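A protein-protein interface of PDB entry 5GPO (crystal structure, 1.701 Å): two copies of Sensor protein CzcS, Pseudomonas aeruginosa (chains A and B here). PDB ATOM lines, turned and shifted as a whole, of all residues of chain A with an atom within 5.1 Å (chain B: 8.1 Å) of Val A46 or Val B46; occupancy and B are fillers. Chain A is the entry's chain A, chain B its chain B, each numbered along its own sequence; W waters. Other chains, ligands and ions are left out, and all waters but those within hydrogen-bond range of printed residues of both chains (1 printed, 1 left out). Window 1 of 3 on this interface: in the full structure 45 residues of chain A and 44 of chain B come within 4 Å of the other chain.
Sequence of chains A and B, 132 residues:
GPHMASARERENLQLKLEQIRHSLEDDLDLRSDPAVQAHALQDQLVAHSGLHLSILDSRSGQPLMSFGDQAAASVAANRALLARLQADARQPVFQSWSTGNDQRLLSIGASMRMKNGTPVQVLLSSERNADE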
ATOM      1  N   GLN A  42     -24.460 -19.261   0.251  1.00  0.00           N
ATOM      2  CA  GLN A  42     -23.025 -19.338   0.008  1.00  0.00           C
ATOM      3  C   GLN A  42     -22.309 -20.143   1.094  1.00  0.00           C
ATOM      4  O   GLN A  42     -21.485 -21.014   0.793  1.00  0.00           O
ATOM      5  CB  GLN A  42     -22.469 -17.923  -0.084  1.00  0.00           C
ATOM      6  CG  GLN A  42     -21.001 -17.843  -0.323  1.00  0.00           C
ATOM      7  CD  GLN A  42     -20.572 -16.453  -0.707  1.00  0.00           C
ATOM      8  OE1 GLN A  42     -20.444 -16.129  -1.897  1.00  0.00           O
ATOM      9  NE2 GLN A  42     -20.370 -15.605   0.293  1.00  0.00           N
ATOM     10  N   ASP A  43     -22.635 -19.886   2.365  1.00  0.00           N
ATOM     11  CA  ASP A  43     -22.017 -20.658   3.447  1.00  0.00           C
ATOM     12  C   ASP A  43     -22.265 -22.157   3.278  1.00  0.00           C
ATOM     13  O   ASP A  43     -21.378 -22.975   3.544  1.00  0.00           O
ATOM     14  CB  ASP A  43     -22.534 -20.189   4.809  1.00  0.00           C
ATOM     15  CG  ASP A  43     -22.081 -18.779   5.173  1.00  0.00           C
ATOM     16  OD1 ASP A  43     -21.036 -18.308   4.670  1.00  0.00           O
ATOM     17  OD2 ASP A  43     -22.784 -18.139   5.979  1.00  0.00           O
ATOM     18  N   GLN A  44     -23.469 -22.549   2.838  1.00  0.00           N
ATOM     19  CA  GLN A  44     -23.741 -23.975   2.711  1.00  0.00           C
ATOM     20  C   GLN A  44     -23.028 -24.585   1.507  1.00  0.00           C
ATOM     21  O   GLN A  44     -22.656 -25.764   1.541  1.00  0.00           O
ATOM     22  CB  GLN A  44     -25.247 -24.222   2.622  1.00  0.00           C
ATOM     23  CG  GLN A  44     -25.625 -25.702   2.479  1.00  0.00           C
ATOM     24  CD  GLN A  44     -25.300 -26.510   3.730  1.00  0.00           C
ATOM     25  OE1 GLN A  44     -25.130 -27.728   3.669  1.00  0.00           O
ATOM     26  NE2 GLN A  44     -25.221 -25.833   4.874  1.00  0.00           N
ATOM     27  N   LEU A  45     -22.854 -23.818   0.430  1.00  0.00           N
ATOM     28  CA  LEU A  45     -22.099 -24.317  -0.717  1.00  0.00           C
ATOM     29  C   LEU A  45     -20.635 -24.549  -0.347  1.00  0.00           C
ATOM     30  O   LEU A  45     -20.036 -25.563  -0.730  1.00  0.00           O
ATOM     31  CB  LEU A  45     -22.211 -23.342  -1.899  1.00  0.00           C
ATOM     32  CG  LEU A  45     -21.668 -23.867  -3.245  1.00  0.00           C
ATOM     33  CD1 LEU A  45     -22.516 -24.981  -3.841  1.00  0.00           C
ATOM     34  CD2 LEU A  45     -21.474 -22.753  -4.259  1.00  0.00           C
ATOM     35  N   VAL A  46     -20.040 -23.628   0.409  1.00  0.00           N
ATOM     36  CA  VAL A  46     -18.635 -23.815   0.750  1.00  0.00           C
ATOM     37  C   VAL A  46     -18.463 -24.866   1.843  1.00  0.00           C
ATOM     38  O   VAL A  46     -17.395 -25.497   1.927  1.00  0.00           O
ATOM     39  CB  VAL A  46     -18.010 -22.452   1.114  1.00  0.00           C
ATOM     40  CG1 VAL A  46     -18.640 -21.885   2.343  1.00  0.00           C
ATOM     41  CG2 VAL A  46     -16.502 -22.574   1.296  1.00  0.00           C
ATOM     42  N   ALA A  47     -19.512 -25.114   2.646  1.00  0.00           N
ATOM     43  CA  ALA A  47     -19.434 -26.069   3.747  1.00  0.00           C
ATOM     44  C   ALA A  47     -19.259 -27.496   3.268  1.00  0.00           C
ATOM     45  O   ALA A  47     -18.857 -28.350   4.064  1.00  0.00           O
ATOM     46  CB  ALA A  47     -20.684 -25.992   4.633  1.00  0.00           C
ATOM     47  N   HIS A  48     -19.533 -27.779   1.994  1.00  0.00           N
ATOM     48  CA  HIS A  48     -19.334 -29.129   1.482  1.00  0.00           C
ATOM     49  C   HIS A  48     -18.540 -29.113   0.182  1.00  0.00           C
ATOM     50  O   HIS A  48     -18.638 -30.038  -0.643  1.00  0.00           O
ATOM     51  CB  HIS A  48     -20.675 -29.843   1.335  1.00  0.00           C
ATOM     52  CG  HIS A  48     -21.408 -29.967   2.635  1.00  0.00           C
ATOM     53  ND1 HIS A  48     -21.024 -30.845   3.628  1.00  0.00           N
ATOM     54  CD2 HIS A  48     -22.456 -29.273   3.134  1.00  0.00           C
ATOM     55  CE1 HIS A  48     -21.824 -30.704   4.672  1.00  0.00           C
ATOM     56  NE2 HIS A  48     -22.692 -29.744   4.406  1.00  0.00           N
ATOM     57  N   SER A  49     -17.689 -28.096   0.036  1.00  0.00           N
ATOM     58  CA  SER A  49     -16.830 -27.905  -1.123  1.00  0.00           C
ATOM     59  C   SER A  49     -15.540 -28.710  -1.056  1.00  0.00           C
ATOM     60  O   SER A  49     -14.822 -28.764  -2.061  1.00  0.00           O
ATOM     61  CB  SER A  49     -16.463 -26.426  -1.248  1.00  0.00           C
ATOM     62  OG  SER A  49     -15.744 -25.994  -0.091  1.00  0.00           O
ATOM     63  N   GLY A  50     -15.225 -29.326   0.083  1.00  0.00           N
ATOM     64  CA  GLY A  50     -13.944 -29.987   0.220  1.00  0.00           C
ATOM     65  C   GLY A  50     -12.779 -29.072   0.552  1.00  0.00           C
ATOM     66  O   GLY A  50     -11.635 -29.525   0.521  1.00  0.00           O
ATOM     67  N   LEU A  51     -13.031 -27.798   0.827  1.00  0.00           N
ATOM     68  CA  LEU A  51     -12.000 -26.800   1.074  1.00  0.00           C
ATOM     69  C   LEU A  51     -12.227 -26.200   2.449  1.00  0.00           C
ATOM     70  O   LEU A  51     -13.368 -25.948   2.837  1.00  0.00           O
ATOM     71  CB  LEU A  51     -12.046 -25.675   0.034  1.00  0.00           C
ATOM     72  CG  LEU A  51     -11.803 -25.994  -1.441  1.00  0.00           C
ATOM     73  CD1 LEU A  51     -12.027 -24.746  -2.277  1.00  0.00           C
ATOM     74  CD2 LEU A  51     -10.381 -26.507  -1.638  1.00  0.00           C
ATOM     75  N   GLY A  68     -15.367 -22.914   5.862  1.00  0.00           N
ATOM     76  CA  GLY A  68     -15.422 -23.962   4.858  1.00  0.00           C
ATOM     77  C   GLY A  68     -15.817 -25.339   5.352  1.00  0.00           C
ATOM     78  O   GLY A  68     -16.596 -25.462   6.298  1.00  0.00           O
ATOM     79  N   ASP A  69     -15.261 -26.370   4.712  1.00  0.00           N
ATOM     80  CA  ASP A  69     -15.697 -27.753   4.856  1.00  0.00           C
ATOM     81  C   ASP A  69     -14.978 -28.370   6.053  1.00  0.00           C
ATOM     82  O   ASP A  69     -13.756 -28.562   6.021  1.00  0.00           O
ATOM     83  CB  ASP A  69     -15.407 -28.526   3.563  1.00  0.00           C
ATOM     84  CG  ASP A  69     -16.209 -29.804   3.430  1.00  0.00           C
ATOM     85  OD1 ASP A  69     -16.592 -30.388   4.464  1.00  0.00           O
ATOM     86  OD2 ASP A  69     -16.453 -30.228   2.268  1.00  0.00           O
ATOM     87  N   ILE B  20      -6.319 -16.196  -2.474  1.00  0.00           N
ATOM     88  CA  ILE B  20      -6.630 -15.686  -1.141  1.00  0.00           C
ATOM     89  C   ILE B  20      -5.714 -14.523  -0.780  1.00  0.00           C
ATOM     90  O   ILE B  20      -6.159 -13.526  -0.200  1.00  0.00           O
ATOM     91  CB  ILE B  20      -6.545 -16.814  -0.097  1.00  0.00           C
ATOM     92  CG1 ILE B  20      -7.646 -17.837  -0.360  1.00  0.00           C
ATOM     93  CG2 ILE B  20      -6.700 -16.237   1.299  1.00  0.00           C
ATOM     94  CD1 ILE B  20      -7.465 -19.134   0.384  1.00  0.00           C
ATOM     95  N   HIS B  39     -15.069 -11.437   6.053  1.00  0.00           N
ATOM     96  CA  HIS B  39     -16.087 -11.504   5.012  1.00  0.00           C
ATOM     97  C   HIS B  39     -15.465 -11.584   3.621  1.00  0.00           C
ATOM     98  O   HIS B  39     -15.955 -12.318   2.753  1.00  0.00           O
ATOM     99  CB  HIS B  39     -17.005 -10.294   5.123  1.00  0.00           C
ATOM    100  CG  HIS B  39     -18.136 -10.322   4.154  1.00  0.00           C
ATOM    101  ND1 HIS B  39     -19.349 -10.901   4.451  1.00  0.00           N
ATOM    102  CD2 HIS B  39     -18.229  -9.877   2.880  1.00  0.00           C
ATOM    103  CE1 HIS B  39     -20.147 -10.802   3.404  1.00  0.00           C
ATOM    104  NE2 HIS B  39     -19.494 -10.180   2.439  1.00  0.00           N
ATOM    105  N   ALA B  40     -14.387 -10.833   3.386  1.00  0.00           N
ATOM    106  CA  ALA B  40     -13.732 -10.876   2.082  1.00  0.00           C
ATOM    107  C   ALA B  40     -13.127 -12.251   1.809  1.00  0.00           C
ATOM    108  O   ALA B  40     -13.223 -12.771   0.692  1.00  0.00           O
ATOM    109  CB  ALA B  40     -12.654  -9.793   2.003  1.00  0.00           C
ATOM    110  N   LEU B  41     -12.488 -12.849   2.813  1.00  0.00           N
ATOM    111  CA  LEU B  41     -11.897 -14.172   2.619  1.00  0.00           C
ATOM    112  C   LEU B  41     -12.968 -15.220   2.348  1.00  0.00           C
ATOM    113  O   LEU B  41     -12.793 -16.097   1.488  1.00  0.00           O
ATOM    114  CB  LEU B  41     -11.083 -14.558   3.847  1.00  0.00           C
ATOM    115  CG  LEU B  41      -9.855 -13.689   4.033  1.00  0.00           C
ATOM    116  CD1 LEU B  41      -9.159 -14.034   5.350  1.00  0.00           C
ATOM    117  CD2 LEU B  41      -8.954 -13.914   2.843  1.00  0.00           C
ATOM    118  N   GLN B  42     -14.085 -15.142   3.066  1.00  0.00           N
ATOM    119  CA  GLN B  42     -15.146 -16.119   2.852  1.00  0.00           C
ATOM    120  C   GLN B  42     -15.741 -15.983   1.455  1.00  0.00           C
ATOM    121  O   GLN B  42     -16.032 -16.990   0.796  1.00  0.00           O
ATOM    122  CB  GLN B  42     -16.215 -15.971   3.934  1.00  0.00           C
ATOM    123  CG  GLN B  42     -17.427 -16.918   3.806  1.00  0.00           C
ATOM    124  CD  GLN B  42     -17.106 -18.386   4.103  1.00  0.00           C
ATOM    125  OE1 GLN B  42     -16.071 -18.911   3.691  1.00  0.00           O
ATOM    126  NE2 GLN B  42     -17.996 -19.044   4.828  1.00  0.00           N
ATOM    127  N   ASP B  43     -15.905 -14.751   0.970  1.00  0.00           N
ATOM    128  CA  ASP B  43     -16.423 -14.580  -0.383  1.00  0.00           C
ATOM    129  C   ASP B  43     -15.443 -15.120  -1.413  1.00  0.00           C
ATOM    130  O   ASP B  43     -15.854 -15.712  -2.418  1.00  0.00           O
ATOM    131  CB  ASP B  43     -16.752 -13.110  -0.657  1.00  0.00           C
ATOM    132  CG  ASP B  43     -18.094 -12.697  -0.084  1.00  0.00           C
ATOM    133  OD1 ASP B  43     -18.651 -13.438   0.757  1.00  0.00           O
ATOM    134  OD2 ASP B  43     -18.597 -11.623  -0.475  1.00  0.00           O
ATOM    135  N   GLN B  44     -14.142 -14.960  -1.168  1.00  0.00           N
ATOM    136  CA  GLN B  44     -13.152 -15.415  -2.133  1.00  0.00           C
ATOM    137  C   GLN B  44     -13.002 -16.936  -2.127  1.00  0.00           C
ATOM    138  O   GLN B  44     -12.691 -17.524  -3.172  1.00  0.00           O
ATOM    139  CB  GLN B  44     -11.798 -14.757  -1.862  1.00  0.00           C
ATOM    140  CG  GLN B  44     -10.710 -15.147  -2.868  1.00  0.00           C
ATOM    141  CD  GLN B  44     -10.845 -14.437  -4.215  1.00  0.00           C
ATOM    142  OE1 GLN B  44     -11.945 -14.273  -4.749  1.00  0.00           O
ATOM    143  NE2 GLN B  44      -9.716 -14.015  -4.771  1.00  0.00           N
ATOM    144  N   LEU B  45     -13.198 -17.588  -0.973  1.00  0.00           N
ATOM    145  CA  LEU B  45     -13.125 -19.047  -0.946  1.00  0.00           C
ATOM    146  C   LEU B  45     -14.171 -19.662  -1.878  1.00  0.00           C
ATOM    147  O   LEU B  45     -13.880 -20.613  -2.613  1.00  0.00           O
ATOM    148  CB  LEU B  45     -13.291 -19.553   0.485  1.00  0.00           C
ATOM    149  CG  LEU B  45     -12.987 -21.037   0.713  1.00  0.00           C
ATOM    150  CD1 LEU B  45     -11.589 -21.375   0.258  1.00  0.00           C
ATOM    151  CD2 LEU B  45     -13.199 -21.448   2.158  1.00  0.00           C
ATOM    152  N   VAL B  46     -15.379 -19.102  -1.881  1.00  0.00           N
ATOM    153  CA  VAL B  46     -16.455 -19.568  -2.754  1.00  0.00           C
ATOM    154  C   VAL B  46     -16.115 -19.320  -4.214  1.00  0.00           C
ATOM    155  O   VAL B  46     -16.440 -20.127  -5.095  1.00  0.00           O
ATOM    156  CB  VAL B  46     -17.762 -18.861  -2.355  1.00  0.00           C
ATOM    157  CG1 VAL B  46     -18.944 -19.405  -3.154  1.00  0.00           C
ATOM    158  CG2 VAL B  46     -17.955 -18.989  -0.847  1.00  0.00           C
ATOM    159  N   ALA B  47     -15.437 -18.209  -4.492  1.00  0.00           N
ATOM    160  CA  ALA B  47     -15.193 -17.808  -5.870  1.00  0.00           C
ATOM    161  C   ALA B  47     -14.267 -18.763  -6.605  1.00  0.00           C
ATOM    162  O   ALA B  47     -14.212 -18.724  -7.835  1.00  0.00           O
ATOM    163  CB  ALA B  47     -14.631 -16.386  -5.905  1.00  0.00           C
ATOM    164  N   HIS B  48     -13.555 -19.635  -5.894  1.00  0.00           N
ATOM    165  CA  HIS B  48     -12.686 -20.594  -6.560  1.00  0.00           C
ATOM    166  C   HIS B  48     -12.892 -21.996  -5.999  1.00  0.00           C
ATOM    167  O   HIS B  48     -12.005 -22.850  -6.080  1.00  0.00           O
ATOM    168  CB  HIS B  48     -11.233 -20.120  -6.480  1.00  0.00           C
ATOM    169  CG  HIS B  48     -11.048 -18.733  -7.030  1.00  0.00           C
ATOM    170  ND1 HIS B  48     -10.903 -18.482  -8.379  1.00  0.00           N
ATOM    171  CD2 HIS B  48     -11.064 -17.524  -6.421  1.00  0.00           C
ATOM    172  CE1 HIS B  48     -10.799 -17.179  -8.572  1.00  0.00           C
ATOM    173  NE2 HIS B  48     -10.896 -16.574  -7.401  1.00  0.00           N
ATOM    174  N   SER B  49     -14.094 -22.253  -5.481  1.00  0.00           N
ATOM    175  CA  SER B  49     -14.515 -23.541  -4.945  1.00  0.00           C
ATOM    176  C   SER B  49     -14.778 -24.599  -6.012  1.00  0.00           C
ATOM    177  O   SER B  49     -15.076 -25.739  -5.654  1.00  0.00           O
ATOM    178  CB  SER B  49     -15.779 -23.358  -4.110  1.00  0.00           C
ATOM    179  OG  SER B  49     -16.861 -23.075  -4.986  1.00  0.00           O
ATOM    180  N   GLY B  50     -14.695 -24.263  -7.299  1.00  0.00           N
ATOM    181  CA  GLY B  50     -15.026 -25.215  -8.344  1.00  0.00           C
ATOM    182  C   GLY B  50     -16.504 -25.516  -8.466  1.00  0.00           C
ATOM    183  O   GLY B  50     -16.887 -26.450  -9.171  1.00  0.00           O
ATOM    184  N   LEU B  51     -17.338 -24.743  -7.793  1.00  0.00           N
ATOM    185  CA  LEU B  51     -18.775 -24.914  -7.808  1.00  0.00           C
ATOM    186  C   LEU B  51     -19.411 -23.565  -8.114  1.00  0.00           C
ATOM    187  O   LEU B  51     -18.868 -22.512  -7.764  1.00  0.00           O
ATOM    188  CB  LEU B  51     -19.255 -25.470  -6.460  1.00  0.00           C
ATOM    189  CG  LEU B  51     -18.740 -26.826  -5.979  1.00  0.00           C
ATOM    190  CD1 LEU B  51     -18.897 -26.907  -4.478  1.00  0.00           C
ATOM    191  CD2 LEU B  51     -19.535 -27.953  -6.644  1.00  0.00           C
ATOM    192  N   HIS B  52     -20.544 -23.591  -8.811  1.00  0.00           N
ATOM    193  CA  HIS B  52     -21.272 -22.361  -9.066  1.00  0.00           C
ATOM    194  C   HIS B  52     -22.757 -22.616  -8.855  1.00  0.00           C
ATOM    195  O   HIS B  52     -23.261 -23.696  -9.178  1.00  0.00           O
ATOM    196  CB  HIS B  52     -21.015 -21.836 -10.482  1.00  0.00           C
ATOM    197  CG  HIS B  52     -21.603 -20.479 -10.732  1.00  0.00           C
ATOM    198  ND1 HIS B  52     -22.896 -20.302 -11.171  1.00  0.00           N
ATOM    199  CD2 HIS B  52     -21.080 -19.236 -10.594  1.00  0.00           C
ATOM    200  CE1 HIS B  52     -23.146 -19.009 -11.304  1.00  0.00           C
ATOM    201  NE2 HIS B  52     -22.061 -18.339 -10.955  1.00  0.00           N
ATOM    202  N   LEU B  53     -23.441 -21.647  -8.263  1.00  0.00           N
ATOM    203  CA  LEU B  53     -24.862 -21.817  -7.979  1.00  0.00           C
ATOM    204  C   LEU B  53     -25.656 -20.645  -8.527  1.00  0.00           C
ATOM    205  O   LEU B  53     -25.340 -19.483  -8.238  1.00  0.00           O
ATOM    206  CB  LEU B  53     -25.099 -21.975  -6.476  1.00  0.00           C
ATOM    207  CG  LEU B  53     -26.553 -22.210  -6.028  1.00  0.00           C
ATOM    208  CD1 LEU B  53     -27.151 -23.427  -6.731  1.00  0.00           C
ATOM    209  CD2 LEU B  53     -26.618 -22.378  -4.518  1.00  0.00           C
ATOM    210  N   SER B  66     -26.667 -15.555  -7.412  1.00  0.00           N
ATOM    211  CA  SER B  66     -25.642 -16.110  -8.278  1.00  0.00           C
ATOM    212  C   SER B  66     -24.309 -15.961  -7.558  1.00  0.00           C
ATOM    213  O   SER B  66     -23.968 -14.852  -7.142  1.00  0.00           O
ATOM    214  CB  SER B  66     -25.635 -15.386  -9.624  1.00  0.00           C
ATOM    215  OG  SER B  66     -24.652 -15.915 -10.485  1.00  0.00           O
ATOM    216  N   PHE B  67     -23.590 -17.069  -7.357  1.00  0.00           N
ATOM    217  CA  PHE B  67     -22.258 -16.983  -6.767  1.00  0.00           C
ATOM    218  C   PHE B  67     -21.486 -18.273  -7.025  1.00  0.00           C
ATOM    219  O   PHE B  67     -22.049 -19.295  -7.408  1.00  0.00           O
ATOM    220  CB  PHE B  67     -22.328 -16.689  -5.263  1.00  0.00           C
ATOM    221  CG  PHE B  67     -23.289 -17.563  -4.515  1.00  0.00           C
ATOM    222  CD1 PHE B  67     -22.942 -18.859  -4.157  1.00  0.00           C
ATOM    223  CD2 PHE B  67     -24.538 -17.086  -4.150  1.00  0.00           C
ATOM    224  CE1 PHE B  67     -23.822 -19.665  -3.454  1.00  0.00           C
ATOM    225  CE2 PHE B  67     -25.428 -17.885  -3.450  1.00  0.00           C
ATOM    226  CZ  PHE B  67     -25.068 -19.177  -3.096  1.00  0.00           C
ATOM    227  N   GLY B  68     -20.180 -18.208  -6.785  1.00  0.00           N
ATOM    228  CA  GLY B  68     -19.338 -19.367  -6.980  1.00  0.00           C
ATOM    229  C   GLY B  68     -18.251 -19.097  -7.994  1.00  0.00           C
ATOM    230  O   GLY B  68     -17.896 -17.942  -8.265  1.00  0.00           O
ATOM    231  N   ASP B  69     -17.772 -20.176  -8.595  1.00  0.00           N
ATOM    232  CA  ASP B  69     -16.592 -20.211  -9.447  1.00  0.00           C
ATOM    233  C   ASP B  69     -17.002 -20.072 -10.915  1.00  0.00           C
ATOM    234  O   ASP B  69     -17.798 -20.867 -11.417  1.00  0.00           O
ATOM    235  CB  ASP B  69     -15.877 -21.541  -9.200  1.00  0.00           C
ATOM    236  CG  ASP B  69     -14.460 -21.571  -9.722  1.00  0.00           C
ATOM    237  OD1 ASP B  69     -14.193 -20.965 -10.788  1.00  0.00           O
ATOM    238  OD2 ASP B  69     -13.631 -22.245  -9.059  1.00  0.00           O
ATOM    239  N   GLN B  70     -16.448 -19.083 -11.619  1.00  0.00           N
ATOM    240  CA  GLN B  70     -16.805 -18.971 -13.032  1.00  0.00           C
ATOM    241  C   GLN B  70     -16.197 -20.090 -13.867  1.00  0.00           C
ATOM    242  O   GLN B  70     -16.687 -20.360 -14.965  1.00  0.00           O
ATOM    243  CB  GLN B  70     -16.387 -17.617 -13.605  1.00  0.00           C
ATOM    244  CG  GLN B  70     -17.445 -16.504 -13.452  1.00  0.00           C
ATOM    245  CD  GLN B  70     -18.749 -16.744 -14.200  1.00  0.00           C
ATOM    246  OE1 GLN B  70     -18.760 -17.291 -15.302  1.00  0.00           O
ATOM    247  NE2 GLN B  70     -19.869 -16.330 -13.590  1.00  0.00           N
ATOM    248  N   ALA B  72     -16.592 -23.031 -13.114  1.00  0.00           N
ATOM    249  CA  ALA B  72     -17.645 -24.034 -13.072  1.00  0.00           C
ATOM    250  C   ALA B  72     -18.921 -23.596 -13.780  1.00  0.00           C
ATOM    251  O   ALA B  72     -19.894 -24.354 -13.787  1.00  0.00           O
ATOM    252  CB  ALA B  72     -17.966 -24.407 -11.615  1.00  0.00           C
HETATM  253  O   HOH W   1     -18.715 -14.902  -3.171  1.00  0.00           O
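Hydrophobic or aromatic side chains of chain B within 4 Å of the printed part of chain A: Leu B45, Val B46 and Phe B67. Printed residues of chain A that touch a printed residue of chain B: Gln A42, Asp A43, Leu A45, Val A46 and Leu A51. Hydrophobic or aromatic side chains of chain A that line the printed part of chain B: Leu A45, Val A46 and Leu A51. Among the printed residues, 9 pairs touch across the chains.
The side-chain hydroxyl of Ser A49 sits at hydrogen-bond distance from the backbone carbonyl oxygen of Val A46 (2.7 Å). The side-chain hydroxyl of Ser A49 lies close to the backbone NH of Leu A51 (3.4 Å). O of Leu A51 lies within hydrogen-bond range of N of Asp A69 (2.7 Å). The side-chain hydroxyl (OG) of Ser B49 is in hydrogen-bond range of the backbone carbonyl oxygen (O) of Val B46, 3.0 Å away. The backbone NH (N) of Leu B51 lies close to the side-chain hydroxyl (OG) of Ser B49 (3.3 Å). The backbone carbonyl oxygen (O) of Phe B67 is in hydrogen-bond range of the backbone NH (N) of Leu B53 (2.9 Å).
Water W1 lies within hydrogen-bond range of OE1 of Gln A42 and O of Asp B43.
CG2 of Val B46 touches CG of Gln A42, 3.3 Å away. Phe B67 touches Gln A42. Phe B67 touches Leu A45 (CE1 to CD2, 3.96 Å). Gln B42 touches Val A46 (NE2 to CG1, 3.8 Å). Val A46 touches Leu B45 (CG2 to CD2, 3.6 Å). Val A46 touches Val B46. Ser B49 touches Leu A51 (CA to CD1, 3.8 Å).
Of the printed residues of chain A, Val B46 touches Gln A42 and Val A46. No residue of chain B comes within 4 Å of Ala A47. Printed residues of chain B within 4 Å of Asp A43: Gln B42. Of the printed residues of chain B, Leu A51 touches Ser B49. Printed residues of chain A within 4 Å of Asp B43: Gln A42. Printed residues of chain A within 4 Å of Leu B45: Val A46. Of the printed residues of chain B, Gln A42 touches Asp B43, Val B46 and Phe B67. The nearest printed residue of chain B that does not touch Val A46 is Ser B49 (5.5 Å).
Gln A42 touches Asp B43, and with the chains exchanged Asp A43 touches Gln B42. Gln A42 touches Val B46, and with the chains exchanged Val A46 touches Gln B42. Val A46 touches Leu B45, but with the chains exchanged Leu A45 does not touch Val B46 (4.3 Å). Leu A51 touches Ser B49, but with the chains exchanged Ser A49 does not touch Leu B51 (4.1 Å).
NE2 of Gln A42 lies within hydrogen-bond range of OD1 of Asp B43 (2.8 Å). OD1 of Asp A43 lies within hydrogen-bond range of NE2 of Gln B42, at 3.1 Å.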
